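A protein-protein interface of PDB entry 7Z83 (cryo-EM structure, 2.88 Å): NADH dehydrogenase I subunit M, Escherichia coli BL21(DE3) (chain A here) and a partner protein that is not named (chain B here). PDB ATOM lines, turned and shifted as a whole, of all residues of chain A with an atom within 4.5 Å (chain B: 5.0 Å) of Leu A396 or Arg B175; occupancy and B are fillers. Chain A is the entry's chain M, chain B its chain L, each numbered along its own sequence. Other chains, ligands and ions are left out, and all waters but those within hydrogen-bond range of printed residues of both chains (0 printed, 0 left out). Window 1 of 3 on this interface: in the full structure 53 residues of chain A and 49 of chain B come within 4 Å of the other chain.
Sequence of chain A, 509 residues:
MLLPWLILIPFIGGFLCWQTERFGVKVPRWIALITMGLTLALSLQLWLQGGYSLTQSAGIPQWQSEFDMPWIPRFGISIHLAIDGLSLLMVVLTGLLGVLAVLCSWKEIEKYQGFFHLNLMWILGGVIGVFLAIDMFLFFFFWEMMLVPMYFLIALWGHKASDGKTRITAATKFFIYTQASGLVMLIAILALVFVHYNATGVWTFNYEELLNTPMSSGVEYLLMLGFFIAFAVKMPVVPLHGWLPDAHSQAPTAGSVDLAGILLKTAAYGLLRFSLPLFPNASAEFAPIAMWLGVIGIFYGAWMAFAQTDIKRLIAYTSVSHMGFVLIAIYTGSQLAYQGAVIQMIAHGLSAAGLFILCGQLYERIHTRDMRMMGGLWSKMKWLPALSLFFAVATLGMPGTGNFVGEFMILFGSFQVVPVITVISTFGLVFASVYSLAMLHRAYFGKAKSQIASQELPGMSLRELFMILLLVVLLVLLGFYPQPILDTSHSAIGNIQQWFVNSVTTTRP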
ATOM      1  N   ALA A 392     -10.316  24.504  20.334  1.00  0.00           N
ATOM      2  CA  ALA A 392      -8.975  25.032  20.552  1.00  0.00           C
ATOM      3  C   ALA A 392      -8.427  24.614  21.909  1.00  0.00           C
ATOM      4  O   ALA A 392      -7.210  24.475  22.068  1.00  0.00           O
ATOM      5  CB  ALA A 392      -8.979  26.553  20.423  1.00  0.00           C
ATOM      6  N   VAL A 393      -9.306  24.416  22.893  1.00  0.00           N
ATOM      7  CA  VAL A 393      -8.904  23.836  24.168  1.00  0.00           C
ATOM      8  C   VAL A 393      -8.488  22.382  23.979  1.00  0.00           C
ATOM      9  O   VAL A 393      -7.534  21.903  24.605  1.00  0.00           O
ATOM     10  CB  VAL A 393     -10.054  24.002  25.182  1.00  0.00           C
ATOM     11  CG1 VAL A 393     -10.094  22.878  26.206  1.00  0.00           C
ATOM     12  CG2 VAL A 393      -9.950  25.349  25.864  1.00  0.00           C
ATOM     13  N   ALA A 394      -9.187  21.664  23.100  1.00  0.00           N
ATOM     14  CA  ALA A 394      -8.825  20.281  22.810  1.00  0.00           C
ATOM     15  C   ALA A 394      -7.458  20.186  22.142  1.00  0.00           C
ATOM     16  O   ALA A 394      -6.662  19.303  22.479  1.00  0.00           O
ATOM     17  CB  ALA A 394      -9.896  19.631  21.937  1.00  0.00           C
ATOM     18  N   THR A 395      -7.152  21.092  21.213  1.00  0.00           N
ATOM     19  CA  THR A 395      -5.881  21.008  20.499  1.00  0.00           C
ATOM     20  C   THR A 395      -4.692  21.564  21.275  1.00  0.00           C
ATOM     21  O   THR A 395      -3.571  21.510  20.759  1.00  0.00           O
ATOM     22  CB  THR A 395      -5.959  21.715  19.140  1.00  0.00           C
ATOM     23  OG1 THR A 395      -5.967  23.135  19.326  1.00  0.00           O
ATOM     24  CG2 THR A 395      -7.171  21.263  18.348  1.00  0.00           C
ATOM     25  N   LEU A 396      -4.882  22.099  22.478  1.00  0.00           N
ATOM     26  CA  LEU A 396      -3.734  22.483  23.291  1.00  0.00           C
ATOM     27  C   LEU A 396      -3.352  21.414  24.305  1.00  0.00           C
ATOM     28  O   LEU A 396      -2.464  21.654  25.130  1.00  0.00           O
ATOM     29  CB  LEU A 396      -3.983  23.820  24.007  1.00  0.00           C
ATOM     30  CG  LEU A 396      -5.198  24.103  24.891  1.00  0.00           C
ATOM     31  CD1 LEU A 396      -4.914  23.785  26.347  1.00  0.00           C
ATOM     32  CD2 LEU A 396      -5.617  25.554  24.750  1.00  0.00           C
ATOM     33  N   GLY A 397      -3.991  20.249  24.263  1.00  0.00           N
ATOM     34  CA  GLY A 397      -3.669  19.176  25.181  1.00  0.00           C
ATOM     35  C   GLY A 397      -4.305  19.355  26.542  1.00  0.00           C
ATOM     36  O   GLY A 397      -3.625  19.272  27.568  1.00  0.00           O
ATOM     37  N   MET A 398      -5.602  19.608  26.563  1.00  0.00           N
ATOM     38  CA  MET A 398      -6.286  19.805  27.835  1.00  0.00           C
ATOM     39  C   MET A 398      -6.924  18.501  28.293  1.00  0.00           C
ATOM     40  O   MET A 398      -7.591  17.835  27.493  1.00  0.00           O
ATOM     41  CB  MET A 398      -7.346  20.891  27.717  1.00  0.00           C
ATOM     42  CG  MET A 398      -8.354  20.926  28.860  1.00  0.00           C
ATOM     43  SD  MET A 398      -7.814  21.815  30.337  1.00  0.00           S
ATOM     44  CE  MET A 398      -6.643  22.991  29.661  1.00  0.00           C
ATOM     45  N   LEU A 429       4.350  21.265  23.935  1.00  0.00           N
ATOM     46  CA  LEU A 429       2.961  21.363  24.392  1.00  0.00           C
ATOM     47  C   LEU A 429       2.653  22.754  24.940  1.00  0.00           C
ATOM     48  O   LEU A 429       1.544  23.280  24.746  1.00  0.00           O
ATOM     49  CB  LEU A 429       2.667  20.306  25.455  1.00  0.00           C
ATOM     50  CG  LEU A 429       2.120  18.949  25.027  1.00  0.00           C
ATOM     51  CD1 LEU A 429       2.209  17.979  26.188  1.00  0.00           C
ATOM     52  CD2 LEU A 429       0.687  19.081  24.548  1.00  0.00           C
ATOM     53  N   VAL A 430       3.617  23.350  25.650  1.00  0.00           N
ATOM     54  CA  VAL A 430       3.475  24.753  26.063  1.00  0.00           C
ATOM     55  C   VAL A 430       3.297  25.657  24.843  1.00  0.00           C
ATOM     56  O   VAL A 430       2.430  26.544  24.826  1.00  0.00           O
ATOM     57  CB  VAL A 430       4.675  25.192  26.930  1.00  0.00           C
ATOM     58  CG1 VAL A 430       4.916  26.689  26.829  1.00  0.00           C
ATOM     59  CG2 VAL A 430       4.412  24.864  28.368  1.00  0.00           C
ATOM     60  N   ALA A 432       2.062  24.764  22.010  1.00  0.00           N
ATOM     61  CA  ALA A 432       0.735  24.466  21.478  1.00  0.00           C
ATOM     62  C   ALA A 432      -0.340  25.275  22.185  1.00  0.00           C
ATOM     63  O   ALA A 432      -1.231  25.850  21.538  1.00  0.00           O
ATOM     64  CB  ALA A 432       0.445  22.971  21.599  1.00  0.00           C
ATOM     65  N   SER A 433      -0.259  25.338  23.518  1.00  0.00           N
ATOM     66  CA  SER A 433      -1.162  26.194  24.280  1.00  0.00           C
ATOM     67  C   SER A 433      -1.014  27.653  23.867  1.00  0.00           C
ATOM     68  O   SER A 433      -2.011  28.382  23.764  1.00  0.00           O
ATOM     69  CB  SER A 433      -0.901  26.033  25.775  1.00  0.00           C
ATOM     70  OG  SER A 433       0.201  26.824  26.180  1.00  0.00           O
ATOM     71  N   SER A 436      -2.744  28.202  20.456  1.00  0.00           N
ATOM     72  CA  SER A 436      -4.193  28.077  20.596  1.00  0.00           C
ATOM     73  C   SER A 436      -4.792  29.322  21.237  1.00  0.00           C
ATOM     74  O   SER A 436      -5.823  29.835  20.776  1.00  0.00           O
ATOM     75  CB  SER A 436      -4.539  26.832  21.412  1.00  0.00           C
ATOM     76  OG  SER A 436      -4.221  25.651  20.702  1.00  0.00           O
ATOM     77  N   GLU B 144      -5.187  21.029  35.453  1.00  0.00           N
ATOM     78  CA  GLU B 144      -5.314  21.725  34.181  1.00  0.00           C
ATOM     79  C   GLU B 144      -6.709  22.298  33.986  1.00  0.00           C
ATOM     80  O   GLU B 144      -6.856  23.335  33.333  1.00  0.00           O
ATOM     81  CB  GLU B 144      -4.958  20.787  33.035  1.00  0.00           C
ATOM     82  CG  GLU B 144      -4.095  21.422  31.960  1.00  0.00           C
ATOM     83  CD  GLU B 144      -2.625  21.435  32.320  1.00  0.00           C
ATOM     84  OE1 GLU B 144      -2.259  20.843  33.355  1.00  0.00           O
ATOM     85  OE2 GLU B 144      -1.830  22.039  31.571  1.00  0.00           O
ATOM     86  N   ALA B 170      -1.122  34.578  32.193  1.00  0.00           N
ATOM     87  CA  ALA B 170      -1.488  33.668  33.273  1.00  0.00           C
ATOM     88  C   ALA B 170      -1.471  32.219  32.807  1.00  0.00           C
ATOM     89  O   ALA B 170      -0.858  31.355  33.449  1.00  0.00           O
ATOM     90  CB  ALA B 170      -2.868  34.035  33.816  1.00  0.00           C
ATOM     91  N   PHE B 171      -2.114  31.940  31.669  1.00  0.00           N
ATOM     92  CA  PHE B 171      -2.180  30.568  31.189  1.00  0.00           C
ATOM     93  C   PHE B 171      -0.820  30.058  30.733  1.00  0.00           C
ATOM     94  O   PHE B 171      -0.523  28.879  30.923  1.00  0.00           O
ATOM     95  CB  PHE B 171      -3.202  30.441  30.064  1.00  0.00           C
ATOM     96  CG  PHE B 171      -3.572  29.019  29.740  1.00  0.00           C
ATOM     97  CD1 PHE B 171      -4.550  28.362  30.465  1.00  0.00           C
ATOM     98  CD2 PHE B 171      -2.941  28.341  28.710  1.00  0.00           C
ATOM     99  CE1 PHE B 171      -4.893  27.058  30.170  1.00  0.00           C
ATOM    100  CE2 PHE B 171      -3.280  27.038  28.410  1.00  0.00           C
ATOM    101  CZ  PHE B 171      -4.256  26.395  29.141  1.00  0.00           C
ATOM    102  N   VAL B 172       0.029  30.919  30.167  1.00  0.00           N
ATOM    103  CA  VAL B 172       1.342  30.458  29.718  1.00  0.00           C
ATOM    104  C   VAL B 172       2.244  30.135  30.908  1.00  0.00           C
ATOM    105  O   VAL B 172       2.929  29.100  30.918  1.00  0.00           O
ATOM    106  CB  VAL B 172       1.980  31.492  28.772  1.00  0.00           C
ATOM    107  CG1 VAL B 172       3.447  31.179  28.534  1.00  0.00           C
ATOM    108  CG2 VAL B 172       1.244  31.504  27.448  1.00  0.00           C
ATOM    109  N   VAL B 173       2.253  30.994  31.936  1.00  0.00           N
ATOM    110  CA  VAL B 173       3.075  30.716  33.114  1.00  0.00           C
ATOM    111  C   VAL B 173       2.573  29.473  33.847  1.00  0.00           C
ATOM    112  O   VAL B 173       3.366  28.597  34.239  1.00  0.00           O
ATOM    113  CB  VAL B 173       3.121  31.948  34.036  1.00  0.00           C
ATOM    114  CG1 VAL B 173       3.807  31.610  35.345  1.00  0.00           C
ATOM    115  CG2 VAL B 173       3.849  33.088  33.349  1.00  0.00           C
ATOM    116  N   THR B 174       1.250  29.349  34.010  1.00  0.00           N
ATOM    117  CA  THR B 174       0.717  28.151  34.647  1.00  0.00           C
ATOM    118  C   THR B 174       0.943  26.911  33.795  1.00  0.00           C
ATOM    119  O   THR B 174       1.127  25.826  34.342  1.00  0.00           O
ATOM    120  CB  THR B 174      -0.768  28.317  34.958  1.00  0.00           C
ATOM    121  OG1 THR B 174      -1.464  28.732  33.781  1.00  0.00           O
ATOM    122  CG2 THR B 174      -0.969  29.348  36.056  1.00  0.00           C
ATOM    123  N   ARG B 175       0.979  27.045  32.466  1.00  0.00           N
ATOM    124  CA  ARG B 175       1.251  25.892  31.616  1.00  0.00           C
ATOM    125  C   ARG B 175       2.707  25.459  31.701  1.00  0.00           C
ATOM    126  O   ARG B 175       3.000  24.264  31.601  1.00  0.00           O
ATOM    127  CB  ARG B 175       0.871  26.203  30.172  1.00  0.00           C
ATOM    128  CG  ARG B 175       0.740  24.973  29.301  1.00  0.00           C
ATOM    129  CD  ARG B 175      -0.644  24.370  29.412  1.00  0.00           C
ATOM    130  NE  ARG B 175      -0.780  23.176  28.590  1.00  0.00           N
ATOM    131  CZ  ARG B 175      -1.905  22.487  28.455  1.00  0.00           C
ATOM    132  NH1 ARG B 175      -3.016  22.854  29.070  1.00  0.00           N
ATOM    133  NH2 ARG B 175      -1.914  21.403  27.687  1.00  0.00           N
ATOM    134  N   VAL B 176       3.630  26.407  31.888  1.00  0.00           N
ATOM    135  CA  VAL B 176       5.018  26.041  32.167  1.00  0.00           C
ATOM    136  C   VAL B 176       5.108  25.279  33.486  1.00  0.00           C
ATOM    137  O   VAL B 176       5.809  24.257  33.595  1.00  0.00           O
ATOM    138  CB  VAL B 176       5.909  27.297  32.170  1.00  0.00           C
ATOM    139  CG1 VAL B 176       7.283  26.982  32.723  1.00  0.00           C
ATOM    140  CG2 VAL B 176       6.024  27.864  30.769  1.00  0.00           C
ATOM    141  N   GLY B 177       4.379  25.752  34.502  1.00  0.00           N
ATOM    142  CA  GLY B 177       4.318  25.016  35.758  1.00  0.00           C
ATOM    143  C   GLY B 177       3.733  23.623  35.603  1.00  0.00           C
ATOM    144  O   GLY B 177       4.229  22.659  36.191  1.00  0.00           O
ATOM    145  N   ASP B 178       2.683  23.493  34.791  1.00  0.00           N
ATOM    146  CA  ASP B 178       2.076  22.188  34.560  1.00  0.00           C
ATOM    147  C   ASP B 178       2.989  21.279  33.752  1.00  0.00           C
ATOM    148  O   ASP B 178       2.931  20.056  33.901  1.00  0.00           O
ATOM    149  CB  ASP B 178       0.727  22.348  33.865  1.00  0.00           C
ATOM    150  CG  ASP B 178      -0.231  23.199  34.663  1.00  0.00           C
ATOM    151  OD1 ASP B 178       0.141  23.598  35.786  1.00  0.00           O
ATOM    152  OD2 ASP B 178      -1.341  23.490  34.174  1.00  0.00           O
ATOM    153  N   VAL B 179       3.851  21.852  32.913  1.00  0.00           N
ATOM    154  CA  VAL B 179       4.849  21.046  32.219  1.00  0.00           C
ATOM    155  C   VAL B 179       5.891  20.522  33.200  1.00  0.00           C
ATOM    156  O   VAL B 179       6.317  19.366  33.107  1.00  0.00           O
ATOM    157  CB  VAL B 179       5.468  21.852  31.063  1.00  0.00           C
ATOM    158  CG1 VAL B 179       6.928  21.492  30.826  1.00  0.00           C
ATOM    159  CG2 VAL B 179       4.676  21.582  29.811  1.00  0.00           C
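The guanidinium group (NH2) of Arg B175 lies within hydrogen-bond range of the backbone carbonyl oxygen (O) of Leu A396 (2.6 Å).
The backbone carbonyl oxygen of Gly A397 lies within hydrogen-bond range of the guanidinium group of Arg B175 (2.7 Å).
SD of Met A398 lies close to O of Glu B144 (3.5 Å).
Of the 12 printed residues of chain A, 5 touch a printed residue of chain B.
Hydrophobic or aromatic side chains of chain A that line the printed part of chain B: Leu A396, Met A398 and Val A430.
Hydrophobic or aromatic side chains of chain B that line the printed part of chain A: Phe B171 and Val B179.
Among the printed residues, 10 pairs touch across the chains.
Among the printed residues, no Asp or Glu carboxylate lies within 4 Å of a Lys or Arg side-chain nitrogen of the other chain.
CD1 of Leu A396 touches CZ of Phe B171, 3.9 Å away.
NH1 of Arg B175 touches CE of Met A398, 3.7 Å away.
CG2 of Val A430 touches O of Arg B175, at 3.6 Å.
CG2 of Val A430 touches N of Val B176 (3.9 Å).
Val B179 touches Val A430 (CG2 to CG2, 3.6 Å).
CE2 of Phe B171 touches CB of Ser A433, 3.7 Å away.
OG of Ser A433 touches CG of Arg B175 (3.7 Å).
NH1 of Arg B175 lies within salt-bridge range of OE2 of Glu B144, 2.9 Å away.
O of Val A430 lies within hydrogen-bond range of OG of Ser A433 (2.6 Å).
The side-chain hydroxyl of Thr B174 sits at hydrogen-bond distance from the backbone carbonyl oxygen of Phe B171 (3.0 Å).
Leu A396 touches just these residues of chain B: Phe B171 (3.9 Å) and Arg B175 (2.6 Å).
Of the printed residues of chain B, Gly A397 touches Arg B175.
Leu A429 touches none of the printed residues of chain B.
Of the printed residues of chain B, Val A430 touches Arg B175, Val B176 and Val B179.
Ala B170 touches none of the printed residues of chain A.
Of the printed residues of chain A, Phe B171 touches Leu A396 (3.9 Å) and Ser A433 (3.7 Å).
Arg B175 touches five residues of chain A.
Of the printed residues of chain A, Val B176 touches Val A430 (3.9 Å).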
